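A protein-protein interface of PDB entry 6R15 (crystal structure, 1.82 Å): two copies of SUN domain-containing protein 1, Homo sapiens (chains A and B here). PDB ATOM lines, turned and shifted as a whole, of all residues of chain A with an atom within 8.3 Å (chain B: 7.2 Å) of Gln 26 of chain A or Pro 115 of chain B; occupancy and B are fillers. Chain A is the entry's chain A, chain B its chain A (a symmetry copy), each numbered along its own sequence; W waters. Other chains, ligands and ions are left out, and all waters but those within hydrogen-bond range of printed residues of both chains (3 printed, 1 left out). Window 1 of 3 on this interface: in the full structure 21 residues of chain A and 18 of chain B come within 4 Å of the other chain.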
ATOM      1  N   SER A  19      16.534  -2.185 -12.482  1.00  0.00           N
ATOM      2  CA  SER A  19      17.821  -1.490 -12.428  1.00  0.00           C
ATOM      3  C   SER A  19      18.907  -2.376 -11.813  1.00  0.00           C
ATOM      4  O   SER A  19      20.067  -2.368 -12.267  1.00  0.00           O
ATOM      5  CB  SER A  19      17.693  -0.195 -11.625  1.00  0.00           C
ATOM      6  OG  SER A  19      17.096   0.837 -12.379  1.00  0.00           O
ATOM      7  N   ALA A  20      18.561  -3.134 -10.773  1.00  0.00           N
ATOM      8  CA  ALA A  20      19.527  -4.054 -10.159  1.00  0.00           C
ATOM      9  C   ALA A  20      19.956  -5.181 -11.102  1.00  0.00           C
ATOM     10  O   ALA A  20      21.153  -5.553 -11.131  1.00  0.00           O
ATOM     11  CB  ALA A  20      18.930  -4.644  -8.870  1.00  0.00           C
ATOM     12  N   LEU A  21      19.009  -5.777 -11.856  1.00  0.00           N
ATOM     13  CA  LEU A  21      19.388  -6.810 -12.834  1.00  0.00           C
ATOM     14  C   LEU A  21      20.214  -6.230 -13.985  1.00  0.00           C
ATOM     15  O   LEU A  21      21.127  -6.903 -14.497  1.00  0.00           O
ATOM     16  CB  LEU A  21      18.138  -7.496 -13.387  1.00  0.00           C
ATOM     17  CG  LEU A  21      17.547  -8.600 -12.512  1.00  0.00           C
ATOM     18  CD1 LEU A  21      16.183  -9.099 -13.084  1.00  0.00           C
ATOM     19  CD2 LEU A  21      18.530  -9.731 -12.473  1.00  0.00           C
ATOM     20  N   LYS A  22      19.948  -4.974 -14.392  1.00  0.00           N
ATOM     21  CA  LYS A  22      20.764  -4.373 -15.451  1.00  0.00           C
ATOM     22  C   LYS A  22      22.230  -4.224 -15.003  1.00  0.00           C
ATOM     23  O   LYS A  22      23.167  -4.584 -15.745  1.00  0.00           O
ATOM     24  CB  LYS A  22      20.151  -3.037 -15.888  1.00  0.00           C
ATOM     25  CG  LYS A  22      20.972  -2.272 -16.934  1.00  0.00           C
ATOM     26  CD  LYS A  22      20.283  -0.933 -17.375  1.00  0.00           C
ATOM     27  CE  LYS A  22      21.126  -0.134 -18.350  1.00  0.00           C
ATOM     28  NZ  LYS A  22      20.327   1.032 -18.877  1.00  0.00           N
ATOM     29  N   LEU A  23      22.464  -3.741 -13.783  1.00  0.00           N
ATOM     30  CA  LEU A  23      23.840  -3.649 -13.289  1.00  0.00           C
ATOM     31  C   LEU A  23      24.481  -5.031 -13.147  1.00  0.00           C
ATOM     32  O   LEU A  23      25.675  -5.211 -13.476  1.00  0.00           O
ATOM     33  CB  LEU A  23      23.862  -2.934 -11.938  1.00  0.00           C
ATOM     34  CG  LEU A  23      25.242  -2.654 -11.320  1.00  0.00           C
ATOM     35  CD1 LEU A  23      25.999  -1.728 -12.254  1.00  0.00           C
ATOM     36  CD2 LEU A  23      25.108  -2.038  -9.897  1.00  0.00           C
ATOM     37  N   TYR A  24      23.715  -6.013 -12.620  1.00  0.00           N
ATOM     38  CA  TYR A  24      24.216  -7.379 -12.470  1.00  0.00           C
ATOM     39  C   TYR A  24      24.725  -7.924 -13.807  1.00  0.00           C
ATOM     40  O   TYR A  24      25.822  -8.522 -13.884  1.00  0.00           O
ATOM     41  CB  TYR A  24      23.112  -8.277 -11.895  1.00  0.00           C
ATOM     42  CG  TYR A  24      23.533  -9.704 -11.530  1.00  0.00           C
ATOM     43  CD1 TYR A  24      24.092  -9.987 -10.288  1.00  0.00           C
ATOM     44  CD2 TYR A  24      23.385 -10.746 -12.422  1.00  0.00           C
ATOM     45  CE1 TYR A  24      24.489 -11.324  -9.929  1.00  0.00           C
ATOM     46  CE2 TYR A  24      23.754 -12.060 -12.100  1.00  0.00           C
ATOM     47  CZ  TYR A  24      24.315 -12.342 -10.851  1.00  0.00           C
ATOM     48  OH  TYR A  24      24.680 -13.658 -10.534  1.00  0.00           O
ATOM     49  N   SER A  25      23.958  -7.704 -14.877  1.00  0.00           N
ATOM     50  CA  SER A  25      24.324  -8.203 -16.195  1.00  0.00           C
ATOM     51  C   SER A  25      25.581  -7.535 -16.775  1.00  0.00           C
ATOM     52  O   SER A  25      26.138  -8.068 -17.758  1.00  0.00           O
ATOM     53  CB  SER A  25      23.154  -8.013 -17.186  1.00  0.00           C
ATOM     54  OG  SER A  25      23.040  -6.647 -17.626  1.00  0.00           O
ATOM     55  N   GLN A  26      26.007  -6.397 -16.240  1.00  0.00           N
ATOM     56  CA  GLN A  26      27.184  -5.673 -16.759  1.00  0.00           C
ATOM     57  C   GLN A  26      28.437  -6.045 -15.970  1.00  0.00           C
ATOM     58  O   GLN A  26      29.069  -5.226 -15.342  1.00  0.00           O
ATOM     59  CB  GLN A  26      26.947  -4.148 -16.719  1.00  0.00           C
ATOM     60  CG  GLN A  26      25.768  -3.710 -17.619  1.00  0.00           C
ATOM     61  CD  GLN A  26      25.597  -2.189 -17.710  1.00  0.00           C
ATOM     62  OE1 GLN A  26      26.285  -1.429 -17.020  1.00  0.00           O
ATOM     63  NE2 GLN A  26      24.684  -1.737 -18.566  1.00  0.00           N
ATOM     64  N   ASP A  27      28.760  -7.340 -15.970  1.00  0.00           N
ATOM     65  CA  ASP A  27      29.919  -7.843 -15.217  1.00  0.00           C
ATOM     66  C   ASP A  27      29.825  -7.484 -13.733  1.00  0.00           C
ATOM     67  O   ASP A  27      30.843  -7.233 -13.086  1.00  0.00           O
ATOM     68  CB  ASP A  27      31.212  -7.306 -15.847  1.00  0.00           C
ATOM     69  CG  ASP A  27      32.448  -8.194 -15.585  1.00  0.00           C
ATOM     70  OD1 ASP A  27      32.328  -9.332 -15.069  1.00  0.00           O
ATOM     71  OD2 ASP A  27      33.582  -7.727 -15.899  1.00  0.00           O
ATOM     72  N   LYS A  28      28.597  -7.476 -13.168  1.00  0.00           N
ATOM     73  CA  LYS A  28      28.278  -7.116 -11.775  1.00  0.00           C
ATOM     74  C   LYS A  28      28.509  -5.657 -11.355  1.00  0.00           C
ATOM     75  O   LYS A  28      27.812  -5.155 -10.468  1.00  0.00           O
ATOM     76  CB  LYS A  28      29.065  -7.995 -10.767  1.00  0.00           C
ATOM     77  CG  LYS A  28      29.132  -9.498 -11.063  1.00  0.00           C
ATOM     78  CD  LYS A  28      27.771 -10.196 -11.078  1.00  0.00           C
ATOM     79  CE  LYS A  28      27.930 -11.752 -11.285  1.00  0.00           C
ATOM     80  NZ  LYS A  28      28.448 -12.105 -12.692  1.00  0.00           N
ATOM     81  N   THR A  29      29.472  -4.963 -11.967  1.00  0.00           N
ATOM     82  CA  THR A  29      29.961  -3.665 -11.510  1.00  0.00           C
ATOM     83  C   THR A  29      29.587  -2.487 -12.397  1.00  0.00           C
ATOM     84  O   THR A  29      29.631  -1.335 -11.942  1.00  0.00           O
ATOM     85  CB  THR A  29      31.508  -3.661 -11.458  1.00  0.00           C
ATOM     86  OG1 THR A  29      31.998  -3.887 -12.803  1.00  0.00           O
ATOM     87  CG2 THR A  29      32.067  -4.735 -10.541  1.00  0.00           C
ATOM     88  N   GLY A  30      29.352  -2.723 -13.683  1.00  0.00           N
ATOM     89  CA  GLY A  30      29.136  -1.621 -14.595  1.00  0.00           C
ATOM     90  C   GLY A  30      30.365  -0.795 -14.935  1.00  0.00           C
ATOM     91  O   GLY A  30      30.224   0.355 -15.340  1.00  0.00           O
ATOM     92  N   MET A  31      31.572  -1.349 -14.772  1.00  0.00           N
ATOM     93  CA  MET A  31      32.830  -0.643 -15.024  1.00  0.00           C
ATOM     94  C   MET A  31      33.733  -1.471 -15.937  1.00  0.00           C
ATOM     95  O   MET A  31      33.801  -2.691 -15.786  1.00  0.00           O
ATOM     96  CB  MET A  31      33.588  -0.380 -13.704  1.00  0.00           C
ATOM     97  CG  MET A  31      32.823   0.406 -12.643  1.00  0.00           C
ATOM     98  SD  MET A  31      33.563   0.224 -10.982  1.00  0.00           S
ATOM     99  CE  MET A  31      35.153   0.960 -11.251  1.00  0.00           C
ATOM    100  N   VAL A  32      34.459  -0.815 -16.850  1.00  0.00           N
ATOM    101  CA  VAL A  32      35.437  -1.526 -17.692  1.00  0.00           C
ATOM    102  C   VAL A  32      36.486  -2.242 -16.838  1.00  0.00           C
ATOM    103  O   VAL A  32      37.039  -1.650 -15.892  1.00  0.00           O
ATOM    104  CB  VAL A  32      36.174  -0.536 -18.618  1.00  0.00           C
ATOM    105  CG1 VAL A  32      37.295  -1.253 -19.415  1.00  0.00           C
ATOM    106  CG2 VAL A  32      35.211   0.167 -19.574  1.00  0.00           C
ATOM    107  N   ASP A  33      36.841  -3.504 -17.238  1.00  0.00           N
ATOM    108  CA  ASP A  33      37.973  -4.249 -16.660  1.00  0.00           C
ATOM    109  C   ASP A  33      39.109  -4.301 -17.696  1.00  0.00           C
ATOM    110  O   ASP A  33      39.045  -5.098 -18.648  1.00  0.00           O
ATOM    111  CB  ASP A  33      37.564  -5.670 -16.263  1.00  0.00           C
ATOM    112  CG  ASP A  33      38.756  -6.510 -15.737  1.00  0.00           C
ATOM    113  OD1 ASP A  33      39.867  -5.927 -15.505  1.00  0.00           O
ATOM    114  OD2 ASP A  33      38.576  -7.738 -15.582  1.00  0.00           O
ATOM    115  N   ARG A 194      39.807 -14.302  -9.518  1.00  0.00           N
ATOM    116  CA  ARG A 194      39.794 -13.247 -10.527  1.00  0.00           C
ATOM    117  C   ARG A 194      40.318 -11.930  -9.945  1.00  0.00           C
ATOM    118  O   ARG A 194      40.002 -11.566  -8.795  1.00  0.00           O
ATOM    119  CB  ARG A 194      38.374 -13.030 -11.118  1.00  0.00           C
ATOM    120  CG  ARG A 194      38.400 -12.015 -12.285  1.00  0.00           C
ATOM    121  CD  ARG A 194      37.180 -12.019 -13.155  1.00  0.00           C
ATOM    122  NE  ARG A 194      37.191 -10.881 -14.068  1.00  0.00           N
ATOM    123  CZ  ARG A 194      36.095 -10.308 -14.550  1.00  0.00           C
ATOM    124  NH1 ARG A 194      34.878 -10.790 -14.272  1.00  0.00           N
ATOM    125  NH2 ARG A 194      36.188  -9.235 -15.342  1.00  0.00           N
ATOM    126  N   ARG A 196      40.735  -7.769 -11.283  1.00  0.00           N
ATOM    127  CA  ARG A 196      40.328  -6.747 -12.252  1.00  0.00           C
ATOM    128  C   ARG A 196      41.018  -5.396 -11.984  1.00  0.00           C
ATOM    129  O   ARG A 196      41.358  -5.068 -10.833  1.00  0.00           O
ATOM    130  CB  ARG A 196      38.792  -6.465 -12.214  1.00  0.00           C
ATOM    131  CG  ARG A 196      37.855  -7.710 -12.185  1.00  0.00           C
ATOM    132  CD  ARG A 196      36.409  -7.272 -12.263  1.00  0.00           C
ATOM    133  NE  ARG A 196      35.478  -8.318 -11.838  1.00  0.00           N
ATOM    134  CZ  ARG A 196      34.173  -8.264 -12.030  1.00  0.00           C
ATOM    135  NH1 ARG A 196      33.652  -7.220 -12.662  1.00  0.00           N
ATOM    136  NH2 ARG A 196      33.398  -9.253 -11.598  1.00  0.00           N
ATOM    137  N   TYR B  24      14.991 -13.645 -16.281  1.00  0.00           N
ATOM    138  CA  TYR B  24      16.410 -13.410 -16.545  1.00  0.00           C
ATOM    139  C   TYR B  24      17.139 -14.728 -16.823  1.00  0.00           C
ATOM    140  O   TYR B  24      17.933 -14.835 -17.784  1.00  0.00           O
ATOM    141  CB  TYR B  24      17.043 -12.673 -15.357  1.00  0.00           C
ATOM    142  CG  TYR B  24      18.493 -12.213 -15.550  1.00  0.00           C
ATOM    143  CD1 TYR B  24      18.778 -10.997 -16.163  1.00  0.00           C
ATOM    144  CD2 TYR B  24      19.553 -12.991 -15.139  1.00  0.00           C
ATOM    145  CE1 TYR B  24      20.134 -10.550 -16.349  1.00  0.00           C
ATOM    146  CE2 TYR B  24      20.885 -12.580 -15.298  1.00  0.00           C
ATOM    147  CZ  TYR B  24      21.169 -11.358 -15.914  1.00  0.00           C
ATOM    148  OH  TYR B  24      22.502 -10.952 -16.068  1.00  0.00           O
ATOM    149  N   ILE B  81      28.777 -12.858 -24.174  1.00  0.00           N
ATOM    150  CA  ILE B  81      28.982 -11.542 -24.792  1.00  0.00           C
ATOM    151  C   ILE B  81      29.895 -10.633 -23.955  1.00  0.00           C
ATOM    152  O   ILE B  81      29.731  -9.398 -23.946  1.00  0.00           O
ATOM    153  CB  ILE B  81      27.644 -10.836 -25.084  1.00  0.00           C
ATOM    154  CG1 ILE B  81      26.840 -10.635 -23.803  1.00  0.00           C
ATOM    155  CG2 ILE B  81      26.840 -11.632 -26.111  1.00  0.00           C
ATOM    156  CD1 ILE B  81      25.748  -9.584 -23.965  1.00  0.00           C
ATOM    157  N   TYR B  82      30.883 -11.217 -23.268  1.00  0.00           N
ATOM    158  CA  TYR B  82      31.946 -10.411 -22.698  1.00  0.00           C
ATOM    159  C   TYR B  82      32.658  -9.652 -23.828  1.00  0.00           C
ATOM    160  O   TYR B  82      32.721 -10.144 -24.970  1.00  0.00           O
ATOM    161  CB  TYR B  82      32.935 -11.301 -21.919  1.00  0.00           C
ATOM    162  CG  TYR B  82      32.435 -11.575 -20.506  1.00  0.00           C
ATOM    163  CD1 TYR B  82      31.478 -12.569 -20.265  1.00  0.00           C
ATOM    164  CD2 TYR B  82      32.855 -10.789 -19.427  1.00  0.00           C
ATOM    165  CE1 TYR B  82      30.975 -12.796 -18.959  1.00  0.00           C
ATOM    166  CE2 TYR B  82      32.337 -11.007 -18.125  1.00  0.00           C
ATOM    167  CZ  TYR B  82      31.395 -11.977 -17.927  1.00  0.00           C
ATOM    168  OH  TYR B  82      30.891 -12.161 -16.682  1.00  0.00           O
ATOM    169  N   PRO B  83      33.191  -8.454 -23.547  1.00  0.00           N
ATOM    170  CA  PRO B  83      33.950  -7.707 -24.566  1.00  0.00           C
ATOM    171  C   PRO B  83      34.951  -8.575 -25.328  1.00  0.00           C
ATOM    172  O   PRO B  83      35.762  -9.297 -24.739  1.00  0.00           O
ATOM    173  CB  PRO B  83      34.668  -6.621 -23.744  1.00  0.00           C
ATOM    174  CG  PRO B  83      33.699  -6.351 -22.568  1.00  0.00           C
ATOM    175  CD  PRO B  83      33.092  -7.711 -22.261  1.00  0.00           C
ATOM    176  N   HIS B 113      24.719  -6.053 -28.393  1.00  0.00           N
ATOM    177  CA  HIS B 113      26.074  -5.493 -28.393  1.00  0.00           C
ATOM    178  C   HIS B 113      26.453  -5.159 -26.946  1.00  0.00           C
ATOM    179  O   HIS B 113      25.578  -5.003 -26.079  1.00  0.00           O
ATOM    180  CB  HIS B 113      26.140  -4.224 -29.256  1.00  0.00           C
ATOM    181  CG  HIS B 113      27.514  -3.844 -29.718  1.00  0.00           C
ATOM    182  ND1 HIS B 113      28.089  -4.365 -30.859  1.00  0.00           N
ATOM    183  CD2 HIS B 113      28.429  -2.997 -29.180  1.00  0.00           C
ATOM    184  CE1 HIS B 113      29.310  -3.868 -30.995  1.00  0.00           C
ATOM    185  NE2 HIS B 113      29.540  -3.033 -29.993  1.00  0.00           N
ATOM    186  N   ILE B 114      27.744  -5.028 -26.661  1.00  0.00           N
ATOM    187  CA  ILE B 114      28.104  -4.644 -25.298  1.00  0.00           C
ATOM    188  C   ILE B 114      27.626  -3.218 -25.019  1.00  0.00           C
ATOM    189  O   ILE B 114      27.509  -2.401 -25.938  1.00  0.00           O
ATOM    190  CB  ILE B 114      29.617  -4.744 -25.025  1.00  0.00           C
ATOM    191  CG1 ILE B 114      30.422  -3.931 -26.047  1.00  0.00           C
ATOM    192  CG2 ILE B 114      30.093  -6.224 -24.969  1.00  0.00           C
ATOM    193  CD1 ILE B 114      31.878  -3.796 -25.603  1.00  0.00           C
ATOM    194  N   PRO B 115      27.367  -2.858 -23.761  1.00  0.00           N
ATOM    195  CA  PRO B 115      27.035  -1.463 -23.447  1.00  0.00           C
ATOM    196  C   PRO B 115      28.284  -0.600 -23.362  1.00  0.00           C
ATOM    197  O   PRO B 115      29.387  -1.087 -23.120  1.00  0.00           O
ATOM    198  CB  PRO B 115      26.344  -1.564 -22.083  1.00  0.00           C
ATOM    199  CG  PRO B 115      26.971  -2.799 -21.441  1.00  0.00           C
ATOM    200  CD  PRO B 115      27.315  -3.737 -22.578  1.00  0.00           C
ATOM    201  N   LYS B 116      28.090   0.714 -23.539  1.00  0.00           N
ATOM    202  CA  LYS B 116      29.217   1.645 -23.508  1.00  0.00           C
ATOM    203  C   LYS B 116      29.979   1.605 -22.191  1.00  0.00           C
ATOM    204  O   LYS B 116      31.196   1.844 -22.171  1.00  0.00           O
ATOM    205  CB  LYS B 116      28.735   3.081 -23.740  1.00  0.00           C
ATOM    206  CG  LYS B 116      28.024   3.287 -25.043  1.00  0.00           C
ATOM    207  CD  LYS B 116      27.486   4.709 -25.165  1.00  0.00           C
ATOM    208  CE  LYS B 116      26.456   4.812 -26.288  1.00  0.00           C
ATOM    209  NZ  LYS B 116      26.030   6.235 -26.515  1.00  0.00           N
ATOM    210  N   THR B 117      29.292   1.345 -21.073  1.00  0.00           N
ATOM    211  CA  THR B 117      29.986   1.331 -19.787  1.00  0.00           C
ATOM    212  C   THR B 117      31.044   0.242 -19.685  1.00  0.00           C
ATOM    213  O   THR B 117      31.849   0.299 -18.752  1.00  0.00           O
ATOM    214  CB  THR B 117      29.009   1.101 -18.634  1.00  0.00           C
ATOM    215  OG1 THR B 117      28.168  -0.038 -18.963  1.00  0.00           O
ATOM    216  CG2 THR B 117      28.196   2.363 -18.384  1.00  0.00           C
ATOM    217  N   LEU B 118      31.000  -0.799 -20.550  1.00  0.00           N
ATOM    218  CA  LEU B 118      32.011  -1.862 -20.530  1.00  0.00           C
ATOM    219  C   LEU B 118      33.004  -1.780 -21.694  1.00  0.00           C
ATOM    220  O   LEU B 118      33.925  -2.606 -21.770  1.00  0.00           O
ATOM    221  CB  LEU B 118      31.341  -3.239 -20.544  1.00  0.00           C
ATOM    222  CG  LEU B 118      30.451  -3.593 -19.339  1.00  0.00           C
ATOM    223  CD1 LEU B 118      29.938  -5.035 -19.479  1.00  0.00           C
ATOM    224  CD2 LEU B 118      31.195  -3.421 -18.033  1.00  0.00           C
ATOM    225  N   SER B 119      32.864  -0.785 -22.568  1.00  0.00           N
ATOM    226  CA  SER B 119      33.781  -0.601 -23.679  1.00  0.00           C
ATOM    227  C   SER B 119      34.927   0.302 -23.254  1.00  0.00           C
ATOM    228  O   SER B 119      34.688   1.394 -22.710  1.00  0.00           O
ATOM    229  CB  SER B 119      33.068   0.011 -24.880  1.00  0.00           C
ATOM    230  OG  SER B 119      33.962   0.053 -25.993  1.00  0.00           O
ATOM    231  N   PRO B 120      36.170  -0.107 -23.471  1.00  0.00           N
ATOM    232  CA  PRO B 120      37.296   0.677 -22.927  1.00  0.00           C
ATOM    233  C   PRO B 120      37.372   2.115 -23.424  1.00  0.00           C
ATOM    234  O   PRO B 120      37.841   2.993 -22.678  1.00  0.00           O
ATOM    235  CB  PRO B 120      38.530  -0.122 -23.363  1.00  0.00           C
ATOM    236  CG  PRO B 120      38.064  -1.051 -24.425  1.00  0.00           C
ATOM    237  CD  PRO B 120      36.607  -1.337 -24.150  1.00  0.00           C
ATOM    238  N   GLY B 122      34.761   4.032 -24.152  1.00  0.00           N
ATOM    239  CA  GLY B 122      33.567   4.791 -23.842  1.00  0.00           C
ATOM    240  C   GLY B 122      32.571   4.921 -24.979  1.00  0.00           C
ATOM    241  O   GLY B 122      31.479   5.483 -24.768  1.00  0.00           O
ATOM    242  N   ASN B 123      32.887   4.398 -26.164  1.00  0.00           N
ATOM    243  CA  ASN B 123      31.947   4.404 -27.278  1.00  0.00           C
ATOM    244  C   ASN B 123      31.809   2.994 -27.833  1.00  0.00           C
ATOM    245  O   ASN B 123      32.653   2.133 -27.603  1.00  0.00           O
ATOM    246  CB  ASN B 123      32.398   5.363 -28.414  1.00  0.00           C
ATOM    247  CG  ASN B 123      33.641   4.866 -29.166  1.00  0.00           C
ATOM    248  OD1 ASN B 123      33.618   3.843 -29.881  1.00  0.00           O
ATOM    249  ND2 ASN B 123      34.730   5.610 -29.028  1.00  0.00           N
ATOM    250  N   ILE B 124      30.759   2.778 -28.613  1.00  0.00           N
ATOM    251  CA  ILE B 124      30.572   1.505 -29.303  1.00  0.00           C
ATOM    252  C   ILE B 124      30.435   1.764 -30.808  1.00  0.00           C
ATOM    253  O   ILE B 124      29.498   1.269 -31.459  1.00  0.00           O
ATOM    254  CB  ILE B 124      29.356   0.744 -28.733  1.00  0.00           C
ATOM    255  CG1 ILE B 124      28.111   1.614 -28.774  1.00  0.00           C
ATOM    256  CG2 ILE B 124      29.645   0.281 -27.301  1.00  0.00           C
ATOM    257  CD1 ILE B 124      26.820   0.852 -28.422  1.00  0.00           C
ATOM    258  N   TYR B 152      19.863  -0.705 -35.304  1.00  0.00           N
ATOM    259  CA  TYR B 152      20.307  -0.896 -33.913  1.00  0.00           C
ATOM    260  C   TYR B 152      20.674   0.480 -33.340  1.00  0.00           C
ATOM    261  O   TYR B 152      21.436   1.236 -33.956  1.00  0.00           O
ATOM    262  CB  TYR B 152      21.495  -1.888 -33.816  1.00  0.00           C
ATOM    263  CG  TYR B 152      21.968  -2.187 -32.371  1.00  0.00           C
ATOM    264  CD1 TYR B 152      21.395  -3.199 -31.601  1.00  0.00           C
ATOM    265  CD2 TYR B 152      22.972  -1.400 -31.766  1.00  0.00           C
ATOM    266  CE1 TYR B 152      21.821  -3.455 -30.251  1.00  0.00           C
ATOM    267  CE2 TYR B 152      23.375  -1.617 -30.415  1.00  0.00           C
ATOM    268  CZ  TYR B 152      22.799  -2.645 -29.679  1.00  0.00           C
ATOM    269  OH  TYR B 152      23.203  -2.857 -28.363  1.00  0.00           O
ATOM    270  N   GLY B 156      20.376   3.007 -27.070  1.00  0.00           N
ATOM    271  CA  GLY B 156      19.416   2.127 -26.420  1.00  0.00           C
ATOM    272  C   GLY B 156      20.066   1.112 -25.494  1.00  0.00           C
ATOM    273  O   GLY B 156      21.203   1.283 -25.036  1.00  0.00           O
ATOM    274  N   GLU B 157      19.306   0.069 -25.168  1.00  0.00           N
ATOM    275  CA  GLU B 157      19.757  -0.994 -24.289  1.00  0.00           C
ATOM    276  C   GLU B 157      20.653  -1.974 -25.045  1.00  0.00           C
ATOM    277  O   GLU B 157      20.628  -2.048 -26.271  1.00  0.00           O
ATOM    278  CB  GLU B 157      18.562  -1.761 -23.708  1.00  0.00           C
ATOM    279  CG  GLU B 157      17.595  -0.906 -22.876  1.00  0.00           C
ATOM    280  CD  GLU B 157      18.193  -0.352 -21.558  1.00  0.00           C
ATOM    281  OE1 GLU B 157      19.248  -0.821 -21.080  1.00  0.00           O
ATOM    282  OE2 GLU B 157      17.587   0.570 -20.978  1.00  0.00           O
ATOM    283  N   SER B 158      21.423  -2.762 -24.286  1.00  0.00           N
ATOM    284  CA  SER B 158      22.326  -3.742 -24.885  1.00  0.00           C
ATOM    285  C   SER B 158      21.583  -4.718 -25.806  1.00  0.00           C
ATOM    286  O   SER B 158      22.016  -4.965 -26.954  1.00  0.00           O
ATOM    287  CB  SER B 158      23.068  -4.476 -23.759  1.00  0.00           C
ATOM    288  OG  SER B 158      23.762  -5.628 -24.224  1.00  0.00           O
HETATM  289  O   HOH W   1      35.275  -4.528 -19.667  1.00  0.00           O
HETATM  290  O   HOH W   2      28.560 -10.361 -17.025  1.00  0.00           O
HETATM  291  O   HOH W   3      31.263 -11.144 -13.421  1.00  0.00           O
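Water W3 lies within hydrogen-bond range of the side-chain carboxylate of Asp 27 of chain A (2.7 Å), the side-chain amino group of Lys 28 of chain A (3.1 Å), the guanidinium group of Arg 196 of chain A (3.4 Å) and the side-chain hydroxyl of Tyr 82 of chain B (3.4 Å).
Water W2 lies within hydrogen-bond range of the side-chain hydroxyl (OH) of Tyr 82 of chain B, the backbone NH (N) of Asp 27 of chain A and the backbone carbonyl oxygen (O) of Ser 25 of chain A.
Water W1 lies within hydrogen-bond range of the backbone NH (N) of Asp 33 of chain A (3.1 Å) and the backbone carbonyl oxygen (O) of Leu 118 of chain B (3.2 Å).
The side-chain hydroxyl of Ser 119 of chain B lies within hydrogen-bond range of the backbone carbonyl oxygen of Asn 123 of chain B, at 2.9 Å.
OG1 of Thr 29 of chain A lies within hydrogen-bond range of N of Met 31 of chain A (3.2 Å).
NH1 of Arg 194 of chain A is in salt-bridge range of OD1 of Asp 27 of chain A.
OH of Tyr 152 of chain B is in hydrogen-bond range of O of Glu 157 of chain B (3.4 Å).
The backbone carbonyl oxygen (O) of Lys 22 of chain A is in hydrogen-bond range of the side-chain hydroxyl (OG) of Ser 25 of chain A (2.8 Å).
NH1 of Arg 196 of chain A is in salt-bridge range of OD2 of Asp 27 of chain A (3.3 Å).
Tyr 24 of chain A touches its own counterpart, Tyr 24 of chain B.
Position printed for both chains: 24.
Of the 15 pairs that touch across the chains among the printed residues, 1 has its exchanged pair printed and touching as well.
Among the printed residues, merely in contact across the chains: Ser 25 of chain A with Tyr 24 of chain B, Val 32 of chain A with Ser 119 of chain B, Asp 27 of chain A with Tyr 82 of chain B, Met 31 of chain A with Leu 118 of chain B, Gly 30 of chain A with Thr 117 of chain B, Val 32 of chain A with Leu 118 of chain B, Tyr 24 of chain A with Tyr 24 of chain B, Met 31 of chain A with Thr 117 of chain B, Gln 26 of chain A with Pro 115 of chain B, Gln 26 of chain A with Leu 118 of chain B, Leu 21 of chain A with Tyr 24 of chain B and Val 32 of chain A with Pro 120 of chain B.
OE1 of Gln 26 of chain A sits at hydrogen-bond distance from OG1 of Thr 117 of chain B (3.0 Å).
N of Val 32 of chain A sits at hydrogen-bond distance from O of Thr 117 of chain B, 3.4 Å away.
The side-chain amino group (NZ) of Lys 22 of chain A lies within salt-bridge range of the side-chain carboxylate (OE1) of Glu 157 of chain B, 3.1 Å away.
Of chain B, only Pro 115 (3.8 Å), Thr 117 (3.0 Å) and Leu 118 (3.9 Å) come within 4 Å of Gln 26 of chain A.
Of chain A, only Gln 26 (3.8 Å) comes within 4 Å of Pro 115 of chain B.
Printed residues of chain A within 4 Å of Glu 157 of chain B: Lys 22 (3.1 Å).
Of the printed residues of chain A, Thr 117 of chain B touches Gln 26 (3.0 Å), Gly 30 (3.6 Å), Met 31 (3.8 Å) and Val 32 (3.4 Å).
Printed residues of chain B within 4 Å of Ser 25 of chain A: Tyr 24 (3.2 Å).
Printed residues of chain B within 4 Å of Leu 21 of chain A: Tyr 24 (3.9 Å).
Of the printed residues of chain B, Val 32 of chain A touches Thr 117 (3.4 Å), Leu 118 (3.6 Å), Ser 119 (3.4 Å) and Pro 120 (3.98 Å).
The nearest printed residue of chain B that does not touch Gly 30 of chain A is Leu 118 of chain B (4.1 Å).
Of the 17 printed residues of chain A, 9 touch a printed residue of chain B.
Along chain A the printed residues that touch a printed residue of chain B span positions 21 to 32.
Of the 19 printed residues of chain B, 8 touch a printed residue of chain A.
Printed residues of chain B that touch a printed residue of chain A: Tyr 24, Tyr 82, Pro 115, Thr 117, Leu 118, Ser 119, Pro 120 and Glu 157.
Among the printed residues, 15 pairs touch across the chains.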
